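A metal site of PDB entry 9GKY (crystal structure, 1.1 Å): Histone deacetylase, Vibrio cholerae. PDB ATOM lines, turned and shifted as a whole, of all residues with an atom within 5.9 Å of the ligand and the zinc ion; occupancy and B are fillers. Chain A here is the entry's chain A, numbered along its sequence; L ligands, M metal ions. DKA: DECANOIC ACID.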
ATOM      1  N   TYR A  21      13.206  26.813  -3.404  1.00  0.00           N
ATOM      2  CA  TYR A  21      14.305  27.284  -2.567  1.00  0.00           C
ATOM      3  C   TYR A  21      13.921  27.372  -1.086  1.00  0.00           C
ATOM      4  O   TYR A  21      14.750  27.127  -0.221  1.00  0.00           O
ATOM      5  CB  TYR A  21      14.929  28.595  -3.072  1.00  0.00           C
ATOM      6  CG  TYR A  21      15.639  28.424  -4.415  1.00  0.00           C
ATOM      7  CD1 TYR A  21      15.925  27.206  -4.995  1.00  0.00           C
ATOM      8  CD2 TYR A  21      16.050  29.565  -5.104  1.00  0.00           C
ATOM      9  CE1 TYR A  21      16.627  27.090  -6.203  1.00  0.00           C
ATOM     10  CE2 TYR A  21      16.738  29.449  -6.309  1.00  0.00           C
ATOM     11  CZ  TYR A  21      17.028  28.242  -6.871  1.00  0.00           C
ATOM     12  OH  TYR A  21      17.722  28.142  -8.052  1.00  0.00           O
ATOM     13  N   LEU A  24      11.672  23.659   1.705  1.00  0.00           N
ATOM     14  CA  LEU A  24      12.201  22.719   2.664  1.00  0.00           C
ATOM     15  C   LEU A  24      11.711  23.052   4.050  1.00  0.00           C
ATOM     16  O   LEU A  24      11.804  24.199   4.473  1.00  0.00           O
ATOM     17  CB  LEU A  24      13.721  22.830   2.567  1.00  0.00           C
ATOM     18  CG  LEU A  24      14.505  21.863   3.429  1.00  0.00           C
ATOM     19  CD1 LEU A  24      14.269  20.481   2.813  1.00  0.00           C
ATOM     20  CD2 LEU A  24      15.937  22.320   3.360  1.00  0.00           C
ATOM     21  N   TYR A  32      19.350  27.316  10.025  1.00  0.00           N
ATOM     22  CA  TYR A  32      19.446  27.792   8.646  1.00  0.00           C
ATOM     23  C   TYR A  32      18.191  28.603   8.286  1.00  0.00           C
ATOM     24  O   TYR A  32      17.041  28.129   8.460  1.00  0.00           O
ATOM     25  CB  TYR A  32      19.623  26.660   7.627  1.00  0.00           C
ATOM     26  CG  TYR A  32      20.073  27.389   6.386  1.00  0.00           C
ATOM     27  CD1 TYR A  32      21.375  27.836   6.244  1.00  0.00           C
ATOM     28  CD2 TYR A  32      19.162  27.797   5.436  1.00  0.00           C
ATOM     29  CE1 TYR A  32      21.767  28.646   5.204  1.00  0.00           C
ATOM     30  CE2 TYR A  32      19.517  28.652   4.423  1.00  0.00           C
ATOM     31  CZ  TYR A  32      20.821  29.074   4.296  1.00  0.00           C
ATOM     32  OH  TYR A  32      21.204  29.964   3.376  1.00  0.00           O
ATOM     33  N   ILE A  34      15.912  29.218   6.153  1.00  0.00           N
ATOM     34  CA  ILE A  34      15.366  28.683   4.927  1.00  0.00           C
ATOM     35  C   ILE A  34      14.362  29.591   4.221  1.00  0.00           C
ATOM     36  O   ILE A  34      14.210  29.477   3.004  1.00  0.00           O
ATOM     37  CB  ILE A  34      14.820  27.259   5.161  1.00  0.00           C
ATOM     38  CG1 ILE A  34      14.533  26.501   3.826  1.00  0.00           C
ATOM     39  CG2 ILE A  34      13.663  27.211   6.138  1.00  0.00           C
ATOM     40  CD1 ILE A  34      15.737  26.375   2.937  1.00  0.00           C
ATOM     41  N   TYR A  37      14.746  32.967   1.060  1.00  0.00           N
ATOM     42  CA  TYR A  37      14.695  33.033  -0.389  1.00  0.00           C
ATOM     43  C   TYR A  37      13.320  33.492  -0.838  1.00  0.00           C
ATOM     44  O   TYR A  37      13.242  34.433  -1.644  1.00  0.00           O
ATOM     45  CB  TYR A  37      15.053  31.658  -0.969  1.00  0.00           C
ATOM     46  CG  TYR A  37      16.390  31.148  -0.431  1.00  0.00           C
ATOM     47  CD1 TYR A  37      17.533  31.739  -0.905  1.00  0.00           C
ATOM     48  CD2 TYR A  37      16.483  30.128   0.517  1.00  0.00           C
ATOM     49  CE1 TYR A  37      18.777  31.382  -0.396  1.00  0.00           C
ATOM     50  CE2 TYR A  37      17.723  29.744   1.009  1.00  0.00           C
ATOM     51  CZ  TYR A  37      18.865  30.381   0.529  1.00  0.00           C
ATOM     52  OH  TYR A  37      20.116  29.987   1.001  1.00  0.00           O
ATOM     53  N   PHE A  98      21.602  19.338   7.877  1.00  0.00           N
ATOM     54  CA  PHE A  98      20.181  19.168   7.593  1.00  0.00           C
ATOM     55  C   PHE A  98      19.782  17.721   7.799  1.00  0.00           C
ATOM     56  O   PHE A  98      20.612  16.811   7.629  1.00  0.00           O
ATOM     57  CB  PHE A  98      19.912  19.482   6.132  1.00  0.00           C
ATOM     58  CG  PHE A  98      20.138  20.930   5.759  1.00  0.00           C
ATOM     59  CD1 PHE A  98      19.401  21.953   6.330  1.00  0.00           C
ATOM     60  CD2 PHE A  98      21.091  21.258   4.805  1.00  0.00           C
ATOM     61  CE1 PHE A  98      19.596  23.258   5.945  1.00  0.00           C
ATOM     62  CE2 PHE A  98      21.282  22.570   4.406  1.00  0.00           C
ATOM     63  CZ  PHE A  98      20.539  23.570   4.981  1.00  0.00           C
ATOM     64  N   LEU A 104      15.228  17.976   0.124  1.00  0.00           N
ATOM     65  CA  LEU A 104      16.558  18.576   0.216  1.00  0.00           C
ATOM     66  C   LEU A 104      17.340  18.343  -1.092  1.00  0.00           C
ATOM     67  O   LEU A 104      18.041  19.247  -1.573  1.00  0.00           O
ATOM     68  CB  LEU A 104      17.338  18.017   1.397  1.00  0.00           C
ATOM     69  CG  LEU A 104      18.759  18.537   1.545  1.00  0.00           C
ATOM     70  CD1 LEU A 104      18.816  20.005   1.832  1.00  0.00           C
ATOM     71  CD2 LEU A 104      19.358  17.796   2.724  1.00  0.00           C
ATOM     72  N   ARG A 107      15.900  20.323  -3.977  1.00  0.00           N
ATOM     73  CA  ARG A 107      16.240  21.718  -3.885  1.00  0.00           C
ATOM     74  C   ARG A 107      17.678  21.977  -4.298  1.00  0.00           C
ATOM     75  O   ARG A 107      17.960  22.915  -5.047  1.00  0.00           O
ATOM     76  CB  ARG A 107      16.105  22.252  -2.462  1.00  0.00           C
ATOM     77  CG  ARG A 107      16.396  23.725  -2.300  1.00  0.00           C
ATOM     78  CD  ARG A 107      16.931  24.098  -0.884  1.00  0.00           C
ATOM     79  NE  ARG A 107      17.155  25.542  -0.797  1.00  0.00           N
ATOM     80  CZ  ARG A 107      18.148  26.239  -1.367  1.00  0.00           C
ATOM     81  NH1 ARG A 107      19.193  25.613  -1.882  1.00  0.00           N
ATOM     82  NH2 ARG A 107      18.013  27.570  -1.432  1.00  0.00           N
ATOM     83  N   SER A 132      19.850  32.386  -4.674  1.00  0.00           N
ATOM     84  CA  SER A 132      20.319  31.307  -3.794  1.00  0.00           C
ATOM     85  C   SER A 132      21.808  31.144  -4.132  1.00  0.00           C
ATOM     86  O   SER A 132      22.445  32.066  -4.611  1.00  0.00           O
ATOM     87  CB  SER A 132      19.563  29.962  -3.936  1.00  0.00           C
ATOM     88  OG  SER A 132      19.838  29.268  -2.680  1.00  0.00           O
ATOM     89  N   GLY A 133      22.344  29.956  -3.847  1.00  0.00           N
ATOM     90  CA  GLY A 133      23.704  29.634  -4.214  1.00  0.00           C
ATOM     91  C   GLY A 133      24.758  30.082  -3.185  1.00  0.00           C
ATOM     92  O   GLY A 133      24.478  30.718  -2.168  1.00  0.00           O
ATOM     93  N   GLY A 134      26.018  29.782  -3.508  1.00  0.00           N
ATOM     94  CA  GLY A 134      27.136  30.037  -2.648  1.00  0.00           C
ATOM     95  C   GLY A 134      27.491  28.937  -1.695  1.00  0.00           C
ATOM     96  O   GLY A 134      27.864  29.213  -0.531  1.00  0.00           O
ATOM     97  N   TYR A 135      27.409  27.681  -2.134  1.00  0.00           N
ATOM     98  CA  TYR A 135      27.549  26.527  -1.268  1.00  0.00           C
ATOM     99  C   TYR A 135      29.022  26.147  -1.178  1.00  0.00           C
ATOM    100  O   TYR A 135      29.421  25.042  -1.565  1.00  0.00           O
ATOM    101  CB  TYR A 135      26.654  25.396  -1.756  1.00  0.00           C
ATOM    102  CG  TYR A 135      25.235  25.830  -2.072  1.00  0.00           C
ATOM    103  CD1 TYR A 135      24.579  26.781  -1.293  1.00  0.00           C
ATOM    104  CD2 TYR A 135      24.550  25.329  -3.171  1.00  0.00           C
ATOM    105  CE1 TYR A 135      23.293  27.223  -1.595  1.00  0.00           C
ATOM    106  CE2 TYR A 135      23.245  25.736  -3.459  1.00  0.00           C
ATOM    107  CZ  TYR A 135      22.637  26.710  -2.692  1.00  0.00           C
ATOM    108  OH  TYR A 135      21.358  27.130  -2.994  1.00  0.00           O
ATOM    109  N   HIS A 136      29.815  27.053  -0.587  1.00  0.00           N
ATOM    110  CA  HIS A 136      31.278  26.999  -0.712  1.00  0.00           C
ATOM    111  C   HIS A 136      31.915  26.011   0.243  1.00  0.00           C
ATOM    112  O   HIS A 136      33.147  25.844   0.119  1.00  0.00           O
ATOM    113  CB  HIS A 136      31.838  28.440  -0.575  1.00  0.00           C
ATOM    114  CG  HIS A 136      31.500  29.075   0.743  1.00  0.00           C
ATOM    115  ND1 HIS A 136      31.966  30.365   1.019  1.00  0.00           N
ATOM    116  CD2 HIS A 136      30.782  28.725   1.816  1.00  0.00           C
ATOM    117  CE1 HIS A 136      31.480  30.740   2.185  1.00  0.00           C
ATOM    118  NE2 HIS A 136      30.751  29.782   2.706  1.00  0.00           N
ATOM    119  N   HIS A 137      31.184  25.370   1.153  1.00  0.00           N
ATOM    120  CA  HIS A 137      31.749  24.406   2.108  1.00  0.00           C
ATOM    121  C   HIS A 137      31.611  22.956   1.646  1.00  0.00           C
ATOM    122  O   HIS A 137      31.989  22.048   2.402  1.00  0.00           O
ATOM    123  CB  HIS A 137      31.128  24.574   3.494  1.00  0.00           C
ATOM    124  CG  HIS A 137      31.280  25.923   4.089  1.00  0.00           C
ATOM    125  ND1 HIS A 137      32.502  26.570   4.186  1.00  0.00           N
ATOM    126  CD2 HIS A 137      30.390  26.707   4.723  1.00  0.00           C
ATOM    127  CE1 HIS A 137      32.277  27.713   4.848  1.00  0.00           C
ATOM    128  NE2 HIS A 137      31.002  27.862   5.173  1.00  0.00           N
ATOM    129  N   GLY A 145      28.740  22.556   6.604  1.00  0.00           N
ATOM    130  CA  GLY A 145      28.303  23.934   6.682  1.00  0.00           C
ATOM    131  C   GLY A 145      27.109  24.257   5.762  1.00  0.00           C
ATOM    132  O   GLY A 145      27.090  25.288   5.093  1.00  0.00           O
ATOM    133  N   PHE A 146      26.108  23.349   5.722  1.00  0.00           N
ATOM    134  CA  PHE A 146      24.869  23.538   5.004  1.00  0.00           C
ATOM    135  C   PHE A 146      25.023  23.397   3.498  1.00  0.00           C
ATOM    136  O   PHE A 146      24.101  23.660   2.738  1.00  0.00           O
ATOM    137  CB  PHE A 146      24.091  24.825   5.346  1.00  0.00           C
ATOM    138  CG  PHE A 146      23.916  25.009   6.818  1.00  0.00           C
ATOM    139  CD1 PHE A 146      23.160  24.108   7.549  1.00  0.00           C
ATOM    140  CD2 PHE A 146      24.459  26.105   7.487  1.00  0.00           C
ATOM    141  CE1 PHE A 146      23.029  24.251   8.929  1.00  0.00           C
ATOM    142  CE2 PHE A 146      24.309  26.233   8.846  1.00  0.00           C
ATOM    143  CZ  PHE A 146      23.578  25.338   9.556  1.00  0.00           C
ATOM    144  N   CYS A 147      26.158  22.799   3.065  1.00  0.00           N
ATOM    145  CA  CYS A 147      26.542  22.647   1.684  1.00  0.00           C
ATOM    146  C   CYS A 147      26.696  21.181   1.302  1.00  0.00           C
ATOM    147  O   CYS A 147      27.434  20.467   1.917  1.00  0.00           O
ATOM    148  CB  CYS A 147      27.842  23.391   1.403  1.00  0.00           C
ATOM    149  SG  CYS A 147      27.760  25.145   1.781  1.00  0.00           S
ATOM    150  N   ASP A 174      31.395  36.185   1.341  1.00  0.00           N
ATOM    151  CA  ASP A 174      30.685  35.639   2.487  1.00  0.00           C
ATOM    152  C   ASP A 174      31.698  35.646   3.634  1.00  0.00           C
ATOM    153  O   ASP A 174      32.921  35.478   3.441  1.00  0.00           O
ATOM    154  CB  ASP A 174      30.182  34.272   2.076  1.00  0.00           C
ATOM    155  CG  ASP A 174      29.463  33.453   3.144  1.00  0.00           C
ATOM    156  OD1 ASP A 174      30.070  33.047   4.159  1.00  0.00           O
ATOM    157  OD2 ASP A 174      28.235  33.192   2.985  1.00  0.00           O
ATOM    158  N   VAL A 175      31.245  35.767   4.894  1.00  0.00           N
ATOM    159  CA  VAL A 175      32.150  35.903   6.043  1.00  0.00           C
ATOM    160  C   VAL A 175      32.970  34.636   6.304  1.00  0.00           C
ATOM    161  O   VAL A 175      34.029  34.725   6.957  1.00  0.00           O
ATOM    162  CB  VAL A 175      31.367  36.270   7.314  1.00  0.00           C
ATOM    163  CG1 VAL A 175      30.659  35.091   7.934  1.00  0.00           C
ATOM    164  CG2 VAL A 175      32.251  36.956   8.361  1.00  0.00           C
ATOM    165  N   HIS A 176      32.538  33.501   5.780  1.00  0.00           N
ATOM    166  CA  HIS A 176      33.197  32.218   5.966  1.00  0.00           C
ATOM    167  C   HIS A 176      34.180  31.950   4.817  1.00  0.00           C
ATOM    168  O   HIS A 176      33.839  32.199   3.664  1.00  0.00           O
ATOM    169  CB  HIS A 176      32.197  31.057   6.097  1.00  0.00           C
ATOM    170  CG  HIS A 176      31.243  31.268   7.215  1.00  0.00           C
ATOM    171  ND1 HIS A 176      29.931  31.741   7.092  1.00  0.00           N
ATOM    172  CD2 HIS A 176      31.410  30.954   8.531  1.00  0.00           C
ATOM    173  CE1 HIS A 176      29.411  31.778   8.310  1.00  0.00           C
ATOM    174  NE2 HIS A 176      30.259  31.335   9.200  1.00  0.00           N
ATOM    175  N   ASP A 251      26.499  37.538   5.750  1.00  0.00           N
ATOM    176  CA  ASP A 251      26.909  37.177   7.090  1.00  0.00           C
ATOM    177  C   ASP A 251      28.122  37.968   7.580  1.00  0.00           C
ATOM    178  O   ASP A 251      28.471  37.829   8.734  1.00  0.00           O
ATOM    179  CB  ASP A 251      27.053  35.686   7.231  1.00  0.00           C
ATOM    180  CG  ASP A 251      27.782  34.920   6.151  1.00  0.00           C
ATOM    181  OD1 ASP A 251      28.406  35.588   5.282  1.00  0.00           O
ATOM    182  OD2 ASP A 251      27.699  33.654   6.246  1.00  0.00           O
ATOM    183  N   GLY A 291      24.614  33.774  -1.289  1.00  0.00           N
ATOM    184  CA  GLY A 291      25.379  33.238  -0.178  1.00  0.00           C
ATOM    185  C   GLY A 291      24.671  33.264   1.172  1.00  0.00           C
ATOM    186  O   GLY A 291      23.435  33.095   1.209  1.00  0.00           O
ATOM    187  N   GLY A 292      25.412  33.371   2.267  1.00  0.00           N
ATOM    188  CA  GLY A 292      24.933  33.139   3.610  1.00  0.00           C
ATOM    189  C   GLY A 292      24.372  34.390   4.288  1.00  0.00           C
ATOM    190  O   GLY A 292      24.134  35.409   3.673  1.00  0.00           O
ATOM    191  N   GLY A 293      24.182  34.232   5.594  1.00  0.00           N
ATOM    192  CA  GLY A 293      23.424  35.158   6.436  1.00  0.00           C
ATOM    193  C   GLY A 293      22.631  34.393   7.498  1.00  0.00           C
ATOM    194  O   GLY A 293      21.994  33.381   7.167  1.00  0.00           O
ATOM    195  N   TYR A 294      22.703  34.842   8.737  1.00  0.00           N
ATOM    196  CA  TYR A 294      22.122  34.100   9.847  1.00  0.00           C
ATOM    197  C   TYR A 294      21.417  35.072  10.768  1.00  0.00           C
ATOM    198  O   TYR A 294      22.049  35.827  11.514  1.00  0.00           O
ATOM    199  CB  TYR A 294      23.225  33.291  10.613  1.00  0.00           C
ATOM    200  CG  TYR A 294      23.810  32.295   9.637  1.00  0.00           C
ATOM    201  CD1 TYR A 294      23.145  31.086   9.413  1.00  0.00           C
ATOM    202  CD2 TYR A 294      24.912  32.587   8.842  1.00  0.00           C
ATOM    203  CE1 TYR A 294      23.532  30.196   8.460  1.00  0.00           C
ATOM    204  CE2 TYR A 294      25.321  31.711   7.852  1.00  0.00           C
ATOM    205  CZ  TYR A 294      24.597  30.536   7.656  1.00  0.00           C
ATOM    206  OH  TYR A 294      24.941  29.631   6.674  1.00  0.00           O
HETATM  207  C1  DKA L   1      27.650  30.088   4.600  1.00  0.00           C
HETATM  208  O1  DKA L   1      26.859  30.781   5.187  1.00  0.00           O
HETATM  209  C2  DKA L   1      27.277  28.675   4.154  1.00  0.00           C
HETATM  210  C3  DKA L   1      25.863  28.353   3.700  1.00  0.00           C
HETATM  211  C4  DKA L   1      25.555  28.864   2.326  1.00  0.00           C
HETATM  212  C5  DKA L   1      24.098  28.668   1.911  1.00  0.00           C
HETATM  213  C6  DKA L   1      23.477  27.347   2.193  1.00  0.00           C
HETATM  214  C7  DKA L   1      22.021  27.142   1.747  1.00  0.00           C
HETATM  215  C8  DKA L   1      21.227  26.056   2.471  1.00  0.00           C
HETATM  216  C9  DKA L   1      19.902  25.817   1.790  1.00  0.00           C
HETATM  217  C10 DKA L   1      19.062  24.639   2.233  1.00  0.00           C
HETATM  218  O2  DKA L   1      28.839  30.413   4.475  1.00  0.00           O
HETATM  219 ZN    ZN M   1      28.832  32.294   5.405  1.00  0.00          ZN
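NE2 of His 137 lies close to O2 of the ligand (3.4 Å).
A ring nitrogen (NE2) of His 136 lies close to an oxygen (O2) of the ligand.
O1 of the ligand sits close to OH of Tyr 294.
A ring nitrogen (NE2) of His 137 sits at hydrogen-bond distance from a ring nitrogen (NE2) of His 136, 3.1 Å away.
O of Gly 145 lies within hydrogen-bond range of SG of Cys 147, 3.4 Å away.
The guanidinium group (NE) of Arg 107 lies within hydrogen-bond range of the backbone carbonyl oxygen (O) of Tyr 21.
SG of Cys 147 sits at hydrogen-bond distance from N of His 137 (3.5 Å).
The side-chain hydroxyl (OH) of Tyr 37 is in hydrogen-bond range of the side-chain hydroxyl (OH) of Tyr 32 (2.6 Å).
The side-chain hydroxyl (OH) of Tyr 135 is in hydrogen-bond range of the guanidinium group (NH1) of Arg 107, at 2.9 Å.
The backbone carbonyl oxygen (O) of Tyr 135 sits close to the side-chain sulfur (SG) of Cys 147 (3.7 Å).
The guanidinium group of Arg 107 lies within hydrogen-bond range of the side-chain hydroxyl of Ser 132 (2.8 Å).
Merely in contact with the ligand: Tyr 32 (3.4 Å), Ile 34 (3.8 Å), Tyr 37 (3.5 Å), Phe 98 (3.3 Å), Arg 107 (3.6 Å), Gly 134 (3.7 Å), Tyr 135 (3.6 Å), Gly 145 (3.5 Å), Phe 146 (3.8 Å) and Gly 292 (3.4 Å).
Hydrophobic or aromatic side chains within 4 Å of the ligand: Tyr 32, Ile 34, Phe 98, Tyr 135, His 136, His 137, His 176 and Tyr 294.
Within 4 Å of the ligand: Tyr 32, Ile 34, Tyr 37, Phe 98, Arg 107, Gly 134, Tyr 135, His 136, His 137, Gly 145, Phe 146, Asp 174, His 176, Asp 251, Gly 292 and Tyr 294.
The nearest printed residue that does not touch the ligand is Leu 24 (4.1 Å).
Of the 25 residues printed, 3 come within 4 Å of the zinc ion.
The nearest printed residue that does not touch the zinc ion is His 136 (4.2 Å).
The zinc ion is bound by the side-chain carboxylate (OD1) of Asp 174 (1.9 Å), the side-chain carboxylate (OD2) of Asp 251 (2.0 Å), a ring nitrogen (ND1) of His 176 (2.1 Å), an oxygen (O2) of the ligand (2.1 Å) and an oxygen (O1) of the ligand (2.5 Å).
The zinc ion has five donor atoms within binding distance.
Slightly farther from the zinc ion lies the side-chain carboxylate (OD2) of Asp 174 (2.6 Å).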
